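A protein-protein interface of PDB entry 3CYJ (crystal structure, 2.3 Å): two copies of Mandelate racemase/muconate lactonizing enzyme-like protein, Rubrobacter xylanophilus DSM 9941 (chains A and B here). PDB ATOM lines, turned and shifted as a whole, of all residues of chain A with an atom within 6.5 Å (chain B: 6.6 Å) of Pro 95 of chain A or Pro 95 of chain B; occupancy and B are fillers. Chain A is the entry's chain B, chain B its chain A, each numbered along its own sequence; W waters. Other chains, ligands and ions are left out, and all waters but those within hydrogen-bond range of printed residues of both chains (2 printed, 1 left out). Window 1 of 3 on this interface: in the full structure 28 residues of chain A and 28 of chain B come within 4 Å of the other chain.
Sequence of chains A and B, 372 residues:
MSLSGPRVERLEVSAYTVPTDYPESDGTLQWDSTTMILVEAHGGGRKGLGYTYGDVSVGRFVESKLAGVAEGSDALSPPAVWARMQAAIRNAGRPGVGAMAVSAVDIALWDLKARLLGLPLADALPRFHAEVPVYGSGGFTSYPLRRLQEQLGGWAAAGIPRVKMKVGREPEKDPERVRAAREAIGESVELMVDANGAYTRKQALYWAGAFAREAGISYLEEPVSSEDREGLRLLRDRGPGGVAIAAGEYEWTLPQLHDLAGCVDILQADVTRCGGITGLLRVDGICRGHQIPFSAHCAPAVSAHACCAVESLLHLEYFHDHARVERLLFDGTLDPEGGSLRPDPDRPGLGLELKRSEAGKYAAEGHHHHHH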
ATOM      1  N   ILE A  89      -4.571  -3.196  18.704  1.00  0.00           N
ATOM      2  CA  ILE A  89      -5.432  -2.090  19.041  1.00  0.00           C
ATOM      3  C   ILE A  89      -5.416  -0.980  17.955  1.00  0.00           C
ATOM      4  O   ILE A  89      -5.786   0.147  18.235  1.00  0.00           O
ATOM      5  CB  ILE A  89      -5.098  -1.535  20.456  1.00  0.00           C
ATOM      6  CG1 ILE A  89      -3.688  -0.910  20.504  1.00  0.00           C
ATOM      7  CG2 ILE A  89      -5.265  -2.677  21.561  1.00  0.00           C
ATOM      8  CD1 ILE A  89      -3.339  -0.247  21.818  1.00  0.00           C
ATOM      9  N   GLY A  93      -7.675   2.175  19.138  1.00  0.00           N
ATOM     10  CA  GLY A  93      -7.114   3.484  19.536  1.00  0.00           C
ATOM     11  C   GLY A  93      -5.826   3.283  20.329  1.00  0.00           C
ATOM     12  O   GLY A  93      -5.848   2.947  21.523  1.00  0.00           O
ATOM     13  N   ARG A  94      -4.716   3.473  19.643  1.00  0.00           N
ATOM     14  CA  ARG A  94      -3.391   3.287  20.196  1.00  0.00           C
ATOM     15  C   ARG A  94      -3.008   4.337  21.229  1.00  0.00           C
ATOM     16  O   ARG A  94      -2.503   3.974  22.272  1.00  0.00           O
ATOM     17  CB  ARG A  94      -2.372   3.313  19.062  1.00  0.00           C
ATOM     18  CG  ARG A  94      -1.403   2.158  19.080  1.00  0.00           C
ATOM     19  CD  ARG A  94      -0.870   2.018  17.681  1.00  0.00           C
ATOM     20  NE  ARG A  94      -1.119   0.722  17.072  1.00  0.00           N
ATOM     21  CZ  ARG A  94      -1.152   0.544  15.755  1.00  0.00           C
ATOM     22  NH1 ARG A  94      -0.964   1.587  14.941  1.00  0.00           N
ATOM     23  NH2 ARG A  94      -1.371  -0.655  15.253  1.00  0.00           N
ATOM     24  N   PRO A  95      -3.228   5.653  20.945  1.00  0.00           N
ATOM     25  CA  PRO A  95      -2.724   6.645  21.911  1.00  0.00           C
ATOM     26  C   PRO A  95      -3.727   6.920  23.003  1.00  0.00           C
ATOM     27  O   PRO A  95      -4.875   6.504  22.885  1.00  0.00           O
ATOM     28  CB  PRO A  95      -2.502   7.869  21.048  1.00  0.00           C
ATOM     29  CG  PRO A  95      -3.614   7.728  19.947  1.00  0.00           C
ATOM     30  CD  PRO A  95      -3.848   6.269  19.757  1.00  0.00           C
ATOM     31  N   GLY A  96      -3.325   7.609  24.066  1.00  0.00           N
ATOM     32  CA  GLY A  96      -4.256   7.909  25.171  1.00  0.00           C
ATOM     33  C   GLY A  96      -4.599   6.666  25.970  1.00  0.00           C
ATOM     34  O   GLY A  96      -3.715   5.951  26.379  1.00  0.00           O
ATOM     35  N   VAL A  97      -5.898   6.392  26.154  1.00  0.00           N
ATOM     36  CA  VAL A  97      -6.369   5.261  26.963  1.00  0.00           C
ATOM     37  C   VAL A  97      -5.712   3.939  26.578  1.00  0.00           C
ATOM     38  O   VAL A  97      -5.222   3.211  27.460  1.00  0.00           O
ATOM     39  CB  VAL A  97      -7.939   5.110  26.911  1.00  0.00           C
ATOM     40  CG1 VAL A  97      -8.346   3.738  27.366  1.00  0.00           C
ATOM     41  CG2 VAL A  97      -8.604   6.193  27.780  1.00  0.00           C
ATOM     42  N   GLY A  98      -5.671   3.635  25.286  1.00  0.00           N
ATOM     43  CA  GLY A  98      -5.069   2.409  24.809  1.00  0.00           C
ATOM     44  C   GLY A  98      -3.608   2.290  25.206  1.00  0.00           C
ATOM     45  O   GLY A  98      -3.167   1.223  25.608  1.00  0.00           O
ATOM     46  N   ALA A  99      -2.843   3.374  25.094  1.00  0.00           N
ATOM     47  CA  ALA A  99      -1.413   3.357  25.383  1.00  0.00           C
ATOM     48  C   ALA A  99      -1.189   3.215  26.897  1.00  0.00           C
ATOM     49  O   ALA A  99      -0.192   2.622  27.320  1.00  0.00           O
ATOM     50  CB  ALA A  99      -0.740   4.663  24.882  1.00  0.00           C
ATOM     51  N   MET A 100      -2.084   3.808  27.696  1.00  0.00           N
ATOM     52  CA  MET A 100      -2.028   3.672  29.159  1.00  0.00           C
ATOM     53  C   MET A 100      -2.314   2.213  29.561  1.00  0.00           C
ATOM     54  O   MET A 100      -1.676   1.657  30.473  1.00  0.00           O
ATOM     55  CB  MET A 100      -3.048   4.604  29.838  1.00  0.00           C
ATOM     56  CG  MET A 100      -2.685   6.143  29.844  1.00  0.00           C
ATOM     57  SD  MET A 100      -4.069   7.319  30.298  1.00  0.00           S
ATOM     58  CE  MET A 100      -4.369   7.931  28.728  1.00  0.00           C
ATOM     59  N   TYR A 250       3.038  13.971  27.079  1.00  0.00           N
ATOM     60  CA  TYR A 250       1.898  13.467  26.237  1.00  0.00           C
ATOM     61  C   TYR A 250       2.264  12.725  24.960  1.00  0.00           C
ATOM     62  O   TYR A 250       1.436  12.489  24.078  1.00  0.00           O
ATOM     63  CB  TYR A 250       0.899  14.580  25.908  1.00  0.00           C
ATOM     64  CG  TYR A 250       0.374  15.182  27.171  1.00  0.00           C
ATOM     65  CD1 TYR A 250      -0.466  14.440  28.022  1.00  0.00           C
ATOM     66  CD2 TYR A 250       0.748  16.468  27.543  1.00  0.00           C
ATOM     67  CE1 TYR A 250      -0.937  14.987  29.212  1.00  0.00           C
ATOM     68  CE2 TYR A 250       0.288  17.031  28.710  1.00  0.00           C
ATOM     69  CZ  TYR A 250      -0.545  16.303  29.556  1.00  0.00           C
ATOM     70  OH  TYR A 250      -0.980  16.895  30.742  1.00  0.00           O
ATOM     71  N   TRP A 252       2.809   9.587  22.993  1.00  0.00           N
ATOM     72  CA  TRP A 252       2.280   8.262  23.198  1.00  0.00           C
ATOM     73  C   TRP A 252       3.145   7.252  22.454  1.00  0.00           C
ATOM     74  O   TRP A 252       3.285   6.100  22.909  1.00  0.00           O
ATOM     75  CB  TRP A 252       0.809   8.186  22.795  1.00  0.00           C
ATOM     76  CG  TRP A 252       0.009   9.231  23.465  1.00  0.00           C
ATOM     77  CD1 TRP A 252      -0.363  10.453  22.938  1.00  0.00           C
ATOM     78  CD2 TRP A 252      -0.538   9.181  24.789  1.00  0.00           C
ATOM     79  NE1 TRP A 252      -1.097  11.157  23.851  1.00  0.00           N
ATOM     80  CE2 TRP A 252      -1.224  10.414  25.001  1.00  0.00           C
ATOM     81  CE3 TRP A 252      -0.528   8.220  25.813  1.00  0.00           C
ATOM     82  CZ2 TRP A 252      -1.918  10.708  26.207  1.00  0.00           C
ATOM     83  CZ3 TRP A 252      -1.191   8.520  27.041  1.00  0.00           C
ATOM     84  CH2 TRP A 252      -1.869   9.766  27.216  1.00  0.00           C
ATOM     85  N   THR A 253       3.771   7.718  21.354  1.00  0.00           N
ATOM     86  CA  THR A 253       4.629   6.833  20.554  1.00  0.00           C
ATOM     87  C   THR A 253       6.066   7.268  20.307  1.00  0.00           C
ATOM     88  O   THR A 253       6.459   8.428  20.495  1.00  0.00           O
ATOM     89  CB  THR A 253       4.034   6.548  19.215  1.00  0.00           C
ATOM     90  OG1 THR A 253       4.064   7.745  18.451  1.00  0.00           O
ATOM     91  CG2 THR A 253       2.619   6.042  19.369  1.00  0.00           C
ATOM     92  N   GLN A 256       6.712  10.093  17.879  1.00  0.00           N
ATOM     93  CA  GLN A 256       6.354  11.440  18.386  1.00  0.00           C
ATOM     94  C   GLN A 256       7.503  11.957  19.201  1.00  0.00           C
ATOM     95  O   GLN A 256       7.900  13.113  19.100  1.00  0.00           O
ATOM     96  CB  GLN A 256       5.140  11.340  19.283  1.00  0.00           C
ATOM     97  CG  GLN A 256       3.819  11.124  18.576  1.00  0.00           C
ATOM     98  CD  GLN A 256       2.686  11.227  19.580  1.00  0.00           C
ATOM     99  OE1 GLN A 256       2.451  10.308  20.397  1.00  0.00           O
ATOM    100  NE2 GLN A 256       2.016  12.394  19.584  1.00  0.00           N
ATOM    101  N   ILE B  89     -10.468  16.550  29.646  1.00  0.00           N
ATOM    102  CA  ILE B  89      -9.870  15.218  29.557  1.00  0.00           C
ATOM    103  C   ILE B  89      -8.323  15.181  29.380  1.00  0.00           C
ATOM    104  O   ILE B  89      -7.767  14.148  29.030  1.00  0.00           O
ATOM    105  CB  ILE B  89     -10.578  14.357  28.494  1.00  0.00           C
ATOM    106  CG1 ILE B  89     -10.296  14.871  27.069  1.00  0.00           C
ATOM    107  CG2 ILE B  89     -12.090  14.259  28.769  1.00  0.00           C
ATOM    108  CD1 ILE B  89     -11.029  14.031  26.058  1.00  0.00           C
ATOM    109  N   ARG B  90      -7.645  16.290  29.666  1.00  0.00           N
ATOM    110  CA  ARG B  90      -6.207  16.392  29.460  1.00  0.00           C
ATOM    111  C   ARG B  90      -5.467  15.210  30.084  1.00  0.00           C
ATOM    112  O   ARG B  90      -4.652  14.558  29.382  1.00  0.00           O
ATOM    113  CB  ARG B  90      -5.646  17.702  30.045  1.00  0.00           C
ATOM    114  CG  ARG B  90      -4.132  17.905  29.810  1.00  0.00           C
ATOM    115  CD  ARG B  90      -3.571  19.025  30.702  1.00  0.00           C
ATOM    116  NE  ARG B  90      -3.214  18.506  32.016  1.00  0.00           N
ATOM    117  CZ  ARG B  90      -2.880  19.260  33.060  1.00  0.00           C
ATOM    118  NH1 ARG B  90      -2.921  20.592  32.952  1.00  0.00           N
ATOM    119  NH2 ARG B  90      -2.564  18.686  34.235  1.00  0.00           N
ATOM    120  N   ALA B  92      -6.939  12.396  31.223  1.00  0.00           N
ATOM    121  CA  ALA B  92      -7.624  11.113  30.996  1.00  0.00           C
ATOM    122  C   ALA B  92      -7.189  10.564  29.628  1.00  0.00           C
ATOM    123  O   ALA B  92      -7.324   9.364  29.340  1.00  0.00           O
ATOM    124  CB  ALA B  92      -9.129  11.282  31.085  1.00  0.00           C
ATOM    125  N   GLY B  93      -6.626  11.439  28.804  1.00  0.00           N
ATOM    126  CA  GLY B  93      -6.114  11.033  27.524  1.00  0.00           C
ATOM    127  C   GLY B  93      -7.034  11.455  26.389  1.00  0.00           C
ATOM    128  O   GLY B  93      -8.112  10.874  26.163  1.00  0.00           O
ATOM    129  N   ARG B  94      -6.585  12.477  25.681  1.00  0.00           N
ATOM    130  CA  ARG B  94      -7.378  13.144  24.692  1.00  0.00           C
ATOM    131  C   ARG B  94      -7.527  12.330  23.397  1.00  0.00           C
ATOM    132  O   ARG B  94      -8.633  12.259  22.823  1.00  0.00           O
ATOM    133  CB  ARG B  94      -6.754  14.521  24.432  1.00  0.00           C
ATOM    134  CG  ARG B  94      -7.700  15.653  24.223  1.00  0.00           C
ATOM    135  CD  ARG B  94      -6.920  16.956  24.309  1.00  0.00           C
ATOM    136  NE  ARG B  94      -7.128  17.642  25.590  1.00  0.00           N
ATOM    137  CZ  ARG B  94      -6.274  18.508  26.117  1.00  0.00           C
ATOM    138  NH1 ARG B  94      -5.135  18.761  25.480  1.00  0.00           N
ATOM    139  NH2 ARG B  94      -6.557  19.116  27.268  1.00  0.00           N
ATOM    140  N   PRO B  95      -6.419  11.712  22.912  1.00  0.00           N
ATOM    141  CA  PRO B  95      -6.479  11.007  21.616  1.00  0.00           C
ATOM    142  C   PRO B  95      -7.029   9.578  21.728  1.00  0.00           C
ATOM    143  O   PRO B  95      -7.117   9.064  22.817  1.00  0.00           O
ATOM    144  CB  PRO B  95      -5.013  10.973  21.179  1.00  0.00           C
ATOM    145  CG  PRO B  95      -4.220  10.977  22.446  1.00  0.00           C
ATOM    146  CD  PRO B  95      -5.089  11.581  23.548  1.00  0.00           C
ATOM    147  N   GLY B  96      -7.348   8.938  20.610  1.00  0.00           N
ATOM    148  CA  GLY B  96      -7.803   7.557  20.621  1.00  0.00           C
ATOM    149  C   GLY B  96      -9.198   7.345  21.229  1.00  0.00           C
ATOM    150  O   GLY B  96     -10.161   8.008  20.849  1.00  0.00           O
ATOM    151  N   VAL B  97      -9.302   6.450  22.205  1.00  0.00           N
ATOM    152  CA  VAL B  97     -10.590   6.190  22.862  1.00  0.00           C
ATOM    153  C   VAL B  97     -11.308   7.495  23.292  1.00  0.00           C
ATOM    154  O   VAL B  97     -12.507   7.626  23.036  1.00  0.00           O
ATOM    155  CB  VAL B  97     -10.394   5.306  24.140  1.00  0.00           C
ATOM    156  CG1 VAL B  97     -11.617   5.429  25.099  1.00  0.00           C
ATOM    157  CG2 VAL B  97     -10.099   3.890  23.743  1.00  0.00           C
ATOM    158  N   GLY B  98     -10.567   8.418  23.948  1.00  0.00           N
ATOM    159  CA  GLY B  98     -11.101   9.698  24.424  1.00  0.00           C
ATOM    160  C   GLY B  98     -11.660  10.551  23.282  1.00  0.00           C
ATOM    161  O   GLY B  98     -12.703  11.248  23.448  1.00  0.00           O
ATOM    162  N   ALA B  99     -10.999  10.500  22.119  1.00  0.00           N
ATOM    163  CA  ALA B  99     -11.407  11.319  20.985  1.00  0.00           C
ATOM    164  C   ALA B  99     -12.653  10.730  20.364  1.00  0.00           C
ATOM    165  O   ALA B  99     -13.540  11.451  19.882  1.00  0.00           O
ATOM    166  CB  ALA B  99     -10.272  11.383  19.923  1.00  0.00           C
ATOM    167  N   MET B 100     -12.685   9.403  20.319  1.00  0.00           N
ATOM    168  CA  MET B 100     -13.840   8.665  19.817  1.00  0.00           C
ATOM    169  C   MET B 100     -15.084   9.004  20.681  1.00  0.00           C
ATOM    170  O   MET B 100     -16.190   9.204  20.147  1.00  0.00           O
ATOM    171  CB  MET B 100     -13.545   7.168  19.844  1.00  0.00           C
ATOM    172  CG  MET B 100     -12.678   6.766  18.699  1.00  0.00           C
ATOM    173  SD  MET B 100     -12.326   5.029  18.453  1.00  0.00           S
ATOM    174  CE  MET B 100     -10.743   5.100  19.145  1.00  0.00           C
ATOM    175  N   TYR B 250      -6.034   8.623  11.633  1.00  0.00           N
ATOM    176  CA  TYR B 250      -5.651   8.507  13.041  1.00  0.00           C
ATOM    177  C   TYR B 250      -5.200   9.768  13.741  1.00  0.00           C
ATOM    178  O   TYR B 250      -4.720   9.679  14.851  1.00  0.00           O
ATOM    179  CB  TYR B 250      -4.579   7.436  13.217  1.00  0.00           C
ATOM    180  CG  TYR B 250      -5.023   6.078  12.697  1.00  0.00           C
ATOM    181  CD1 TYR B 250      -6.069   5.381  13.310  1.00  0.00           C
ATOM    182  CD2 TYR B 250      -4.416   5.502  11.587  1.00  0.00           C
ATOM    183  CE1 TYR B 250      -6.473   4.117  12.824  1.00  0.00           C
ATOM    184  CE2 TYR B 250      -4.811   4.257  11.114  1.00  0.00           C
ATOM    185  CZ  TYR B 250      -5.835   3.574  11.729  1.00  0.00           C
ATOM    186  OH  TYR B 250      -6.238   2.354  11.235  1.00  0.00           O
ATOM    187  N   TRP B 252      -5.398  13.327  15.796  1.00  0.00           N
ATOM    188  CA  TRP B 252      -6.330  13.819  16.805  1.00  0.00           C
ATOM    189  C   TRP B 252      -5.969  15.290  17.225  1.00  0.00           C
ATOM    190  O   TRP B 252      -6.556  15.871  18.135  1.00  0.00           O
ATOM    191  CB  TRP B 252      -6.468  12.786  17.977  1.00  0.00           C
ATOM    192  CG  TRP B 252      -6.140  11.239  17.612  1.00  0.00           C
ATOM    193  CD1 TRP B 252      -4.887  10.696  17.403  1.00  0.00           C
ATOM    194  CD2 TRP B 252      -7.068  10.122  17.457  1.00  0.00           C
ATOM    195  NE1 TRP B 252      -4.988   9.341  17.123  1.00  0.00           N
ATOM    196  CE2 TRP B 252      -6.303   8.972  17.150  1.00  0.00           C
ATOM    197  CE3 TRP B 252      -8.457   9.995  17.524  1.00  0.00           C
ATOM    198  CZ2 TRP B 252      -6.883   7.714  16.934  1.00  0.00           C
ATOM    199  CZ3 TRP B 252      -9.029   8.734  17.298  1.00  0.00           C
ATOM    200  CH2 TRP B 252      -8.242   7.621  16.992  1.00  0.00           C
ATOM    201  N   GLN B 256      -1.591  18.097  13.871  1.00  0.00           N
ATOM    202  CA  GLN B 256      -1.341  16.798  13.214  1.00  0.00           C
ATOM    203  C   GLN B 256      -1.894  16.737  11.779  1.00  0.00           C
ATOM    204  O   GLN B 256      -1.177  16.376  10.852  1.00  0.00           O
ATOM    205  CB  GLN B 256      -1.890  15.633  14.036  1.00  0.00           C
ATOM    206  CG  GLN B 256      -0.964  15.244  15.131  1.00  0.00           C
ATOM    207  CD  GLN B 256      -1.637  14.354  16.137  1.00  0.00           C
ATOM    208  OE1 GLN B 256      -2.755  13.862  15.900  1.00  0.00           O
ATOM    209  NE2 GLN B 256      -0.962  14.133  17.276  1.00  0.00           N
HETATM  210  O   HOH W   1      -6.889   4.878  23.007  1.00  0.00           O
HETATM  211  O   HOH W   2      -7.859   8.306  25.199  1.00  0.00           O
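Gly 93 of chain A touches Met 100 of chain B (CA to CE, 3.99 Å). Pro 95 of chain A touches Gly 96 of chain B. Pro 95 of chain A touches Trp 252 of chain B (CG to NE1, 3.5 Å). N of Gly 96 of chain A touches CG of Pro 95 of chain B, at 3.8 Å. Val 97 of chain A touches Ala 92 of chain B. Val 97 of chain A touches Val 97 of chain B (CB to CB, 3.7 Å). CE of Met 100 of chain A touches O of Ala 92 of chain B, 3.3 Å away. CA of Gly 93 of chain B touches CE of Met 100 of chain A, 3.8 Å away. Pro 95 of chain B touches Trp 252 of chain A.
Of the 13 printed residues of chain A, 7 touch a printed residue of chain B. Printed residues of chain A that touch a printed residue of chain B: Gly 93, Pro 95, Gly 96, Val 97, Met 100, Tyr 250 and Trp 252. Hydrophobic or aromatic side chains of chain A that line the printed part of chain B: Pro 95, Val 97, Met 100, Tyr 250 and Trp 252. Hydrophobic or aromatic side chains of chain B that line the printed part of chain A: Pro 95, Val 97, Met 100 and Trp 252. Among the printed residues, 11 pairs touch across the chains.
Gly 93 of chain A touches Met 100 of chain B, and with the chains exchanged Met 100 of chain A touches Gly 93 of chain B. Pro 95 of chain A touches Gly 96 of chain B, and with the chains exchanged Gly 96 of chain A touches Pro 95 of chain B. Pro 95 of chain A touches Trp 252 of chain B, and with the chains exchanged Trp 252 of chain A touches Pro 95 of chain B. Val 97 of chain A touches its own counterpart, Val 97 of chain B. Positions printed for both chains: 89, 93, 94, 95, 96, 97, 98, 99, 100, 250, 252 and 256. Of the 11 pairs that touch across the chains among the printed residues, 8 have their exchanged pair printed and touching as well.
The side-chain hydroxyl (OH) of Tyr 250 of chain A is in hydrogen-bond range of the guanidinium group (NE) of Arg 90 of chain B, at 3.0 Å. O of Pro 95 of chain B lies close to O of Pro 95 of chain A, 3.4 Å away.
N of Trp 252 of chain B lies within hydrogen-bond range of OE1 of Gln 256 of chain B. O of Tyr 250 of chain A sits at hydrogen-bond distance from NE1 of Trp 252 of chain A, 2.9 Å away. N of Trp 252 of chain A is in hydrogen-bond range of OE1 of Gln 256 of chain A (2.7 Å).
Ile 89 of chain A touches none of the printed residues of chain B. Of the printed residues of chain B, Pro 95 of chain A touches Pro 95 (3.4 Å), Gly 96 (3.8 Å) and Trp 252 (3.5 Å). Ala 99 of chain A touches none of the printed residues of chain B. Of the printed residues of chain A, Ala 92 of chain B touches Val 97 and Met 100. Printed residues of chain A within 4 Å of Gly 93 of chain B: Met 100 (3.8 Å). Of chain A, only Pro 95 (3.4 Å), Gly 96 (3.8 Å) and Trp 252 (3.4 Å) come within 4 Å of Pro 95 of chain B. Of the printed residues of chain A, Val 97 of chain B touches Val 97. The nearest printed residue of chain B that does not touch Pro 95 of chain A is Val 97 of chain B (4.5 Å). The nearest printed residue of chain B that does not touch Val 97 of chain A is Pro 95 of chain B (4.4 Å).
Water W1 lies within hydrogen-bond range of O of Pro 95 of chain A (2.6 Å), O of Gly 93 of chain A (2.6 Å), N of Gly 98 of chain A (2.9 Å) and N of Val 97 of chain B (3.0 Å). Water W2 lies within hydrogen-bond range of O of Pro 95 of chain B (2.6 Å), O of Gly 93 of chain B (2.8 Å), N of Val 97 of chain A (2.9 Å) and N of Gly 98 of chain B (3.0 Å).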
